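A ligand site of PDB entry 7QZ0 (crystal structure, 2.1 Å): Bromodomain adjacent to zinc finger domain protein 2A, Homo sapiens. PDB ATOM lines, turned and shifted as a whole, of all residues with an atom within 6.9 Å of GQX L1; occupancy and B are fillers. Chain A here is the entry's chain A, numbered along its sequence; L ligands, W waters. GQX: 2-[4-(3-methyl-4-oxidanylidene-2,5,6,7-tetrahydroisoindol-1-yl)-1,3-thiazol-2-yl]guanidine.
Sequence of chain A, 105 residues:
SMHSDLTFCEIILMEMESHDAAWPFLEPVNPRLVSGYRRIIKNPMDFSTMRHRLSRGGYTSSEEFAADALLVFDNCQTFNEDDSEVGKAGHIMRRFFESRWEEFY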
ATOM      1  N   TRP A  23      -9.929  25.245 -31.632  1.00  0.00           N
ATOM      2  CA  TRP A  23     -11.003  26.114 -31.183  1.00  0.00           C
ATOM      3  C   TRP A  23     -11.431  25.931 -29.726  1.00  0.00           C
ATOM      4  O   TRP A  23     -11.765  26.926 -29.091  1.00  0.00           O
ATOM      5  CB  TRP A  23     -12.195  25.992 -32.142  1.00  0.00           C
ATOM      6  CG  TRP A  23     -12.836  24.644 -32.187  1.00  0.00           C
ATOM      7  CD1 TRP A  23     -12.610  23.663 -33.103  1.00  0.00           C
ATOM      8  CD2 TRP A  23     -13.849  24.145 -31.307  1.00  0.00           C
ATOM      9  NE1 TRP A  23     -13.397  22.566 -32.831  1.00  0.00           N
ATOM     10  CE2 TRP A  23     -14.174  22.847 -31.729  1.00  0.00           C
ATOM     11  CE3 TRP A  23     -14.505  24.673 -30.186  1.00  0.00           C
ATOM     12  CZ2 TRP A  23     -15.122  22.054 -31.078  1.00  0.00           C
ATOM     13  CZ3 TRP A  23     -15.445  23.885 -29.533  1.00  0.00           C
ATOM     14  CH2 TRP A  23     -15.747  22.595 -29.984  1.00  0.00           C
ATOM     15  N   PRO A  24     -11.442  24.723 -29.122  1.00  0.00           N
ATOM     16  CA  PRO A  24     -11.841  24.659 -27.700  1.00  0.00           C
ATOM     17  C   PRO A  24     -10.835  25.242 -26.754  1.00  0.00           C
ATOM     18  O   PRO A  24     -11.196  25.559 -25.606  1.00  0.00           O
ATOM     19  CB  PRO A  24     -12.003  23.156 -27.446  1.00  0.00           C
ATOM     20  CG  PRO A  24     -11.988  22.502 -28.797  1.00  0.00           C
ATOM     21  CD  PRO A  24     -11.089  23.380 -29.610  1.00  0.00           C
ATOM     22  N   PHE A  25      -9.569  25.397 -27.177  1.00  0.00           N
ATOM     23  CA  PHE A  25      -8.458  25.606 -26.257  1.00  0.00           C
ATOM     24  C   PHE A  25      -7.810  26.968 -26.396  1.00  0.00           C
ATOM     25  O   PHE A  25      -6.766  27.205 -25.770  1.00  0.00           O
ATOM     26  CB  PHE A  25      -7.416  24.510 -26.454  1.00  0.00           C
ATOM     27  CG  PHE A  25      -8.003  23.136 -26.526  1.00  0.00           C
ATOM     28  CD1 PHE A  25      -8.480  22.515 -25.385  1.00  0.00           C
ATOM     29  CD2 PHE A  25      -8.101  22.484 -27.748  1.00  0.00           C
ATOM     30  CE1 PHE A  25      -9.037  21.247 -25.452  1.00  0.00           C
ATOM     31  CE2 PHE A  25      -8.661  21.224 -27.819  1.00  0.00           C
ATOM     32  CZ  PHE A  25      -9.130  20.608 -26.678  1.00  0.00           C
ATOM     33  N   LEU A  26      -8.388  27.869 -27.177  1.00  0.00           N
ATOM     34  CA  LEU A  26      -7.748  29.165 -27.406  1.00  0.00           C
ATOM     35  C   LEU A  26      -7.926  30.123 -26.238  1.00  0.00           C
ATOM     36  O   LEU A  26      -7.147  31.075 -26.109  1.00  0.00           O
ATOM     37  CB  LEU A  26      -8.306  29.813 -28.682  1.00  0.00           C
ATOM     38  CG  LEU A  26      -8.075  29.037 -29.977  1.00  0.00           C
ATOM     39  CD1 LEU A  26      -8.706  29.782 -31.146  1.00  0.00           C
ATOM     40  CD2 LEU A  26      -6.596  28.840 -30.214  1.00  0.00           C
ATOM     41  N   GLU A  27      -8.926  29.911 -25.394  1.00  0.00           N
ATOM     42  CA  GLU A  27      -9.219  30.796 -24.275  1.00  0.00           C
ATOM     43  C   GLU A  27      -9.556  29.941 -23.075  1.00  0.00           C
ATOM     44  O   GLU A  27      -9.962  28.776 -23.227  1.00  0.00           O
ATOM     45  CB  GLU A  27     -10.408  31.727 -24.577  1.00  0.00           C
ATOM     46  CG  GLU A  27     -10.126  32.887 -25.493  1.00  0.00           C
ATOM     47  CD  GLU A  27     -11.229  33.932 -25.401  1.00  0.00           C
ATOM     48  OE1 GLU A  27     -11.553  34.348 -24.265  1.00  0.00           O
ATOM     49  OE2 GLU A  27     -11.766  34.312 -26.457  1.00  0.00           O
ATOM     50  N   PRO A  28      -9.424  30.474 -21.852  1.00  0.00           N
ATOM     51  CA  PRO A  28      -9.855  29.724 -20.669  1.00  0.00           C
ATOM     52  C   PRO A  28     -11.322  29.364 -20.771  1.00  0.00           C
ATOM     53  O   PRO A  28     -12.142  30.159 -21.228  1.00  0.00           O
ATOM     54  CB  PRO A  28      -9.610  30.701 -19.514  1.00  0.00           C
ATOM     55  CG  PRO A  28      -8.577  31.631 -20.017  1.00  0.00           C
ATOM     56  CD  PRO A  28      -8.853  31.786 -21.493  1.00  0.00           C
ATOM     57  N   VAL A  29     -11.663  28.144 -20.339  1.00  0.00           N
ATOM     58  CA  VAL A  29     -13.061  27.788 -20.203  1.00  0.00           C
ATOM     59  C   VAL A  29     -13.731  28.758 -19.241  1.00  0.00           C
ATOM     60  O   VAL A  29     -13.164  29.110 -18.199  1.00  0.00           O
ATOM     61  CB  VAL A  29     -13.202  26.333 -19.724  1.00  0.00           C
ATOM     62  CG1 VAL A  29     -14.652  26.019 -19.397  1.00  0.00           C
ATOM     63  CG2 VAL A  29     -12.636  25.379 -20.764  1.00  0.00           C
ATOM     64  N   ASN A  30     -14.913  29.233 -19.607  1.00  0.00           N
ATOM     65  CA  ASN A  30     -15.677  30.107 -18.733  1.00  0.00           C
ATOM     66  C   ASN A  30     -16.568  29.223 -17.869  1.00  0.00           C
ATOM     67  O   ASN A  30     -17.560  28.685 -18.364  1.00  0.00           O
ATOM     68  CB  ASN A  30     -16.506  31.104 -19.538  1.00  0.00           C
ATOM     69  CG  ASN A  30     -17.206  32.130 -18.674  1.00  0.00           C
ATOM     70  OD1 ASN A  30     -17.355  31.949 -17.467  1.00  0.00           O
ATOM     71  ND2 ASN A  30     -17.658  33.213 -19.286  1.00  0.00           N
ATOM     72  N   LEU A  33     -20.370  29.213 -17.761  1.00  0.00           N
ATOM     73  CA  LEU A  33     -21.099  28.658 -18.887  1.00  0.00           C
ATOM     74  C   LEU A  33     -21.091  27.134 -18.914  1.00  0.00           C
ATOM     75  O   LEU A  33     -21.820  26.538 -19.709  1.00  0.00           O
ATOM     76  CB  LEU A  33     -20.508  29.206 -20.196  1.00  0.00           C
ATOM     77  CG  LEU A  33     -20.569  30.740 -20.327  1.00  0.00           C
ATOM     78  CD1 LEU A  33     -19.781  31.227 -21.542  1.00  0.00           C
ATOM     79  CD2 LEU A  33     -22.009  31.193 -20.430  1.00  0.00           C
ATOM     80  N   VAL A  34     -20.293  26.498 -18.062  1.00  0.00           N
ATOM     81  CA  VAL A  34     -20.054  25.068 -18.130  1.00  0.00           C
ATOM     82  C   VAL A  34     -20.328  24.498 -16.744  1.00  0.00           C
ATOM     83  O   VAL A  34     -19.486  24.596 -15.846  1.00  0.00           O
ATOM     84  CB  VAL A  34     -18.623  24.749 -18.588  1.00  0.00           C
ATOM     85  CG1 VAL A  34     -18.438  23.231 -18.745  1.00  0.00           C
ATOM     86  CG2 VAL A  34     -18.327  25.461 -19.896  1.00  0.00           C
ATOM     87  N   TYR A  37     -17.649  22.546 -14.116  1.00  0.00           N
ATOM     88  CA  TYR A  37     -16.270  22.601 -14.597  1.00  0.00           C
ATOM     89  C   TYR A  37     -15.317  22.971 -13.468  1.00  0.00           C
ATOM     90  O   TYR A  37     -14.238  22.368 -13.327  1.00  0.00           O
ATOM     91  CB  TYR A  37     -16.135  23.591 -15.751  1.00  0.00           C
ATOM     92  CG  TYR A  37     -14.830  23.412 -16.475  1.00  0.00           C
ATOM     93  CD1 TYR A  37     -14.682  22.390 -17.415  1.00  0.00           C
ATOM     94  CD2 TYR A  37     -13.722  24.225 -16.198  1.00  0.00           C
ATOM     95  CE1 TYR A  37     -13.475  22.184 -18.075  1.00  0.00           C
ATOM     96  CE2 TYR A  37     -12.503  24.037 -16.859  1.00  0.00           C
ATOM     97  CZ  TYR A  37     -12.387  23.011 -17.799  1.00  0.00           C
ATOM     98  OH  TYR A  37     -11.210  22.798 -18.466  1.00  0.00           O
ATOM     99  N   ILE A  41     -12.366  20.308 -12.617  1.00  0.00           N
ATOM    100  CA  ILE A  41     -11.047  20.639 -13.154  1.00  0.00           C
ATOM    101  C   ILE A  41     -10.347  21.529 -12.141  1.00  0.00           C
ATOM    102  O   ILE A  41     -10.683  22.711 -12.004  1.00  0.00           O
ATOM    103  CB  ILE A  41     -11.154  21.302 -14.544  1.00  0.00           C
ATOM    104  CG1 ILE A  41     -11.673  20.284 -15.568  1.00  0.00           C
ATOM    105  CG2 ILE A  41      -9.794  21.848 -15.022  1.00  0.00           C
ATOM    106  CD1 ILE A  41     -10.834  18.998 -15.609  1.00  0.00           C
ATOM    107  N   MET A  45      -6.142  25.020 -17.860  1.00  0.00           N
ATOM    108  CA  MET A  45      -5.042  25.481 -18.705  1.00  0.00           C
ATOM    109  C   MET A  45      -5.555  25.570 -20.129  1.00  0.00           C
ATOM    110  O   MET A  45      -6.414  24.804 -20.547  1.00  0.00           O
ATOM    111  CB  MET A  45      -3.828  24.559 -18.611  1.00  0.00           C
ATOM    112  CG  MET A  45      -2.572  25.029 -19.358  1.00  0.00           C
ATOM    113  SD  MET A  45      -1.964  26.674 -18.907  1.00  0.00           S
ATOM    114  CE  MET A  45      -1.731  26.483 -17.141  1.00  0.00           C
ATOM    115  N   VAL A  72      -3.612  20.775 -20.650  1.00  0.00           N
ATOM    116  CA  VAL A  72      -4.766  21.116 -21.486  1.00  0.00           C
ATOM    117  C   VAL A  72      -5.525  19.854 -21.875  1.00  0.00           C
ATOM    118  O   VAL A  72      -6.754  19.773 -21.759  1.00  0.00           O
ATOM    119  CB  VAL A  72      -4.320  21.911 -22.713  1.00  0.00           C
ATOM    120  CG1 VAL A  72      -5.513  22.136 -23.610  1.00  0.00           C
ATOM    121  CG2 VAL A  72      -3.708  23.242 -22.313  1.00  0.00           C
ATOM    122  N   ASN A  75      -7.036  17.727 -18.857  1.00  0.00           N
ATOM    123  CA  ASN A  75      -8.299  18.356 -18.466  1.00  0.00           C
ATOM    124  C   ASN A  75      -9.398  18.020 -19.446  1.00  0.00           C
ATOM    125  O   ASN A  75     -10.514  17.658 -19.061  1.00  0.00           O
ATOM    126  CB  ASN A  75      -8.125  19.872 -18.371  1.00  0.00           C
ATOM    127  CG  ASN A  75      -7.321  20.279 -17.173  1.00  0.00           C
ATOM    128  OD1 ASN A  75      -7.156  19.490 -16.245  1.00  0.00           O
ATOM    129  ND2 ASN A  75      -6.818  21.496 -17.174  1.00  0.00           N
ATOM    130  N   CYS A  76      -9.112  18.146 -20.742  1.00  0.00           N
ATOM    131  CA  CYS A  76     -10.112  17.872 -21.767  1.00  0.00           C
ATOM    132  C   CYS A  76     -10.649  16.445 -21.643  1.00  0.00           C
ATOM    133  O   CYS A  76     -11.866  16.220 -21.683  1.00  0.00           O
ATOM    134  CB  CYS A  76      -9.496  18.093 -23.147  1.00  0.00           C
ATOM    135  SG  CYS A  76     -10.621  17.778 -24.517  1.00  0.00           S
ATOM    136  N   PHE A  79     -12.928  16.024 -18.433  1.00  0.00           N
ATOM    137  CA  PHE A  79     -14.273  16.600 -18.400  1.00  0.00           C
ATOM    138  C   PHE A  79     -15.170  16.138 -19.543  1.00  0.00           C
ATOM    139  O   PHE A  79     -16.389  16.058 -19.345  1.00  0.00           O
ATOM    140  CB  PHE A  79     -14.197  18.131 -18.414  1.00  0.00           C
ATOM    141  CG  PHE A  79     -15.494  18.782 -18.043  1.00  0.00           C
ATOM    142  CD1 PHE A  79     -15.814  18.983 -16.712  1.00  0.00           C
ATOM    143  CD2 PHE A  79     -16.408  19.144 -19.014  1.00  0.00           C
ATOM    144  CE1 PHE A  79     -17.005  19.556 -16.353  1.00  0.00           C
ATOM    145  CE2 PHE A  79     -17.612  19.720 -18.660  1.00  0.00           C
ATOM    146  CZ  PHE A  79     -17.910  19.923 -17.323  1.00  0.00           C
ATOM    147  N   ASN A  80     -14.616  15.856 -20.714  1.00  0.00           N
ATOM    148  CA  ASN A  80     -15.398  15.592 -21.922  1.00  0.00           C
ATOM    149  C   ASN A  80     -15.312  14.129 -22.338  1.00  0.00           C
ATOM    150  O   ASN A  80     -14.231  13.533 -22.323  1.00  0.00           O
ATOM    151  CB  ASN A  80     -14.924  16.480 -23.073  1.00  0.00           C
ATOM    152  CG  ASN A  80     -14.879  17.920 -22.659  1.00  0.00           C
ATOM    153  OD1 ASN A  80     -15.906  18.599 -22.662  1.00  0.00           O
ATOM    154  ND2 ASN A  80     -13.705  18.384 -22.239  1.00  0.00           N
ATOM    155  N   GLU A  85     -17.868  16.709 -29.041  1.00  0.00           N
ATOM    156  CA  GLU A  85     -17.216  17.619 -29.978  1.00  0.00           C
ATOM    157  C   GLU A  85     -15.888  18.104 -29.410  1.00  0.00           C
ATOM    158  O   GLU A  85     -14.855  18.061 -30.091  1.00  0.00           O
ATOM    159  CB  GLU A  85     -18.119  18.805 -30.307  1.00  0.00           C
ATOM    160  CG  GLU A  85     -19.082  18.528 -31.418  1.00  0.00           C
ATOM    161  CD  GLU A  85     -18.371  18.125 -32.701  1.00  0.00           C
ATOM    162  OE1 GLU A  85     -17.414  18.840 -33.095  1.00  0.00           O
ATOM    163  OE2 GLU A  85     -18.757  17.092 -33.289  1.00  0.00           O
ATOM    164  N   VAL A  86     -15.897  18.570 -28.156  1.00  0.00           N
ATOM    165  CA  VAL A  86     -14.666  19.030 -27.546  1.00  0.00           C
ATOM    166  C   VAL A  86     -13.711  17.869 -27.355  1.00  0.00           C
ATOM    167  O   VAL A  86     -12.510  17.980 -27.639  1.00  0.00           O
ATOM    168  CB  VAL A  86     -14.958  19.766 -26.224  1.00  0.00           C
ATOM    169  CG1 VAL A  86     -13.671  20.150 -25.531  1.00  0.00           C
ATOM    170  CG2 VAL A  86     -15.824  21.011 -26.482  1.00  0.00           C
HETATM  171  C10 GQX L   1     -19.373  25.624 -27.283  1.00  0.00           C
HETATM  172  C01 GQX L   1     -11.669  22.904 -23.199  1.00  0.00           C
HETATM  173  C02 GQX L   1     -13.080  23.396 -23.508  1.00  0.00           C
HETATM  174  C04 GQX L   1     -14.709  24.573 -24.433  1.00  0.00           C
HETATM  175  C05 GQX L   1     -15.390  25.548 -25.368  1.00  0.00           C
HETATM  176  C06 GQX L   1     -14.761  26.646 -26.012  1.00  0.00           C
HETATM  177  C08 GQX L   1     -17.145  26.361 -26.698  1.00  0.00           C
HETATM  178  C14 GQX L   1     -15.322  23.707 -23.543  1.00  0.00           C
HETATM  179  C15 GQX L   1     -16.848  23.488 -23.156  1.00  0.00           C
HETATM  180  C16 GQX L   1     -17.100  22.191 -22.380  1.00  0.00           C
HETATM  181  C17 GQX L   1     -16.009  21.699 -21.466  1.00  0.00           C
HETATM  182  C18 GQX L   1     -14.619  21.905 -21.909  1.00  0.00           C
HETATM  183  C20 GQX L   1     -14.296  22.965 -22.953  1.00  0.00           C
HETATM  184  N03 GQX L   1     -13.368  24.367 -24.402  1.00  0.00           N
HETATM  185  N09 GQX L   1     -18.475  26.506 -27.299  1.00  0.00           N
HETATM  186  N11 GQX L   1     -20.655  25.932 -27.905  1.00  0.00           N
HETATM  187  N12 GQX L   1     -19.196  24.313 -26.675  1.00  0.00           N
HETATM  188  N13 GQX L   1     -16.779  25.373 -25.793  1.00  0.00           N
HETATM  189  O19 GQX L   1     -13.731  21.253 -21.458  1.00  0.00           O
HETATM  190  S07 GQX L   1     -15.849  27.321 -26.960  1.00  0.00           S
HETATM  191  C10 GQX L   2     -15.124  31.188 -23.261  1.00  0.00           C
HETATM  192  C01 GQX L   2     -23.124  26.186 -24.002  1.00  0.00           C
HETATM  193  C02 GQX L   2     -21.915  27.085 -24.295  1.00  0.00           C
HETATM  194  C04 GQX L   2     -19.845  27.942 -24.160  1.00  0.00           C
HETATM  195  C05 GQX L   2     -18.412  28.148 -23.675  1.00  0.00           C
HETATM  196  C06 GQX L   2     -17.783  27.282 -22.743  1.00  0.00           C
HETATM  197  C08 GQX L   2     -16.270  29.104 -23.383  1.00  0.00           C
HETATM  198  C14 GQX L   2     -20.530  28.677 -25.143  1.00  0.00           C
HETATM  199  C15 GQX L   2     -20.104  29.895 -26.085  1.00  0.00           C
HETATM  200  C16 GQX L   2     -21.297  30.674 -26.636  1.00  0.00           C
HETATM  201  C17 GQX L   2     -22.406  29.803 -27.151  1.00  0.00           C
HETATM  202  C18 GQX L   2     -22.832  28.709 -26.233  1.00  0.00           C
HETATM  203  C20 GQX L   2     -21.833  28.132 -25.230  1.00  0.00           C
HETATM  204  N03 GQX L   2     -20.708  27.003 -23.671  1.00  0.00           N
HETATM  205  N09 GQX L   2     -15.101  29.964 -23.484  1.00  0.00           N
HETATM  206  N11 GQX L   2     -16.367  31.865 -22.891  1.00  0.00           N
HETATM  207  N12 GQX L   2     -13.896  31.952 -23.385  1.00  0.00           N
HETATM  208  N13 GQX L   2     -17.482  29.245 -24.053  1.00  0.00           N
HETATM  209  O19 GQX L   2     -23.939  28.280 -26.292  1.00  0.00           O
HETATM  210  S07 GQX L   2     -16.312  27.785 -22.433  1.00  0.00           S
HETATM  211  O   HOH W   1      -8.741  24.133 -21.847  1.00  0.00           O
HETATM  212  O   HOH W   2     -11.303  20.844 -20.441  1.00  0.00           O
HETATM  213  O   HOH W   3     -12.677  28.521 -24.258  1.00  0.00           O
HETATM  214  O   HOH W   4     -19.790  21.614 -26.920  1.00  0.00           O
HETATM  215  O   HOH W   5      -8.850  21.340 -21.916  1.00  0.00           O
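The side-chain amide nitrogen of Asn 80 sits at hydrogen-bond distance from an oxygen (O19) of GQX L1 (3.0 Å).
N12 of GQX L2 lies within salt-bridge range of OE1 of Glu 27 (3.5 Å).
N of Asn 30 sits close to S07 of GQX L2, 3.5 Å away.
N03 of GQX L1 is in hydrogen-bond range of O of Pro 24 (2.8 Å).
O of Pro 28 lies within hydrogen-bond range of N12 of GQX L2 (3.3 Å).
O of Cys 76 is in hydrogen-bond range of ND2 of Asn 80, at 2.9 Å.
The backbone carbonyl oxygen (O) of Val 86 is in hydrogen-bond range of the side-chain sulfur (SG) of Cys 76 (3.7 Å).
Merely in contact with GQX L1: Phe 25 (3.8 Å), Val 29 (3.4 Å), Val 34 (3.96 Å), Tyr 37 (3.5 Å), Phe 79 (3.6 Å) and Val 86 (3.9 Å).
Within 4 Å of GQX L1: Pro 24, Phe 25, Val 29, Val 34, Tyr 37, Phe 79, Asn 80 and Val 86.
Along chain A the residues within 4 Å of GQX L1 span positions 24 to 86.
The nearest printed residue that does not touch GQX L1 is Trp 23 (4.1 Å).
Water W2 lies within hydrogen-bond range of O19 of GQX L1 (2.7 Å), OH of Tyr 37 (2.8 Å) and N of Cys 76 (3.5 Å).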
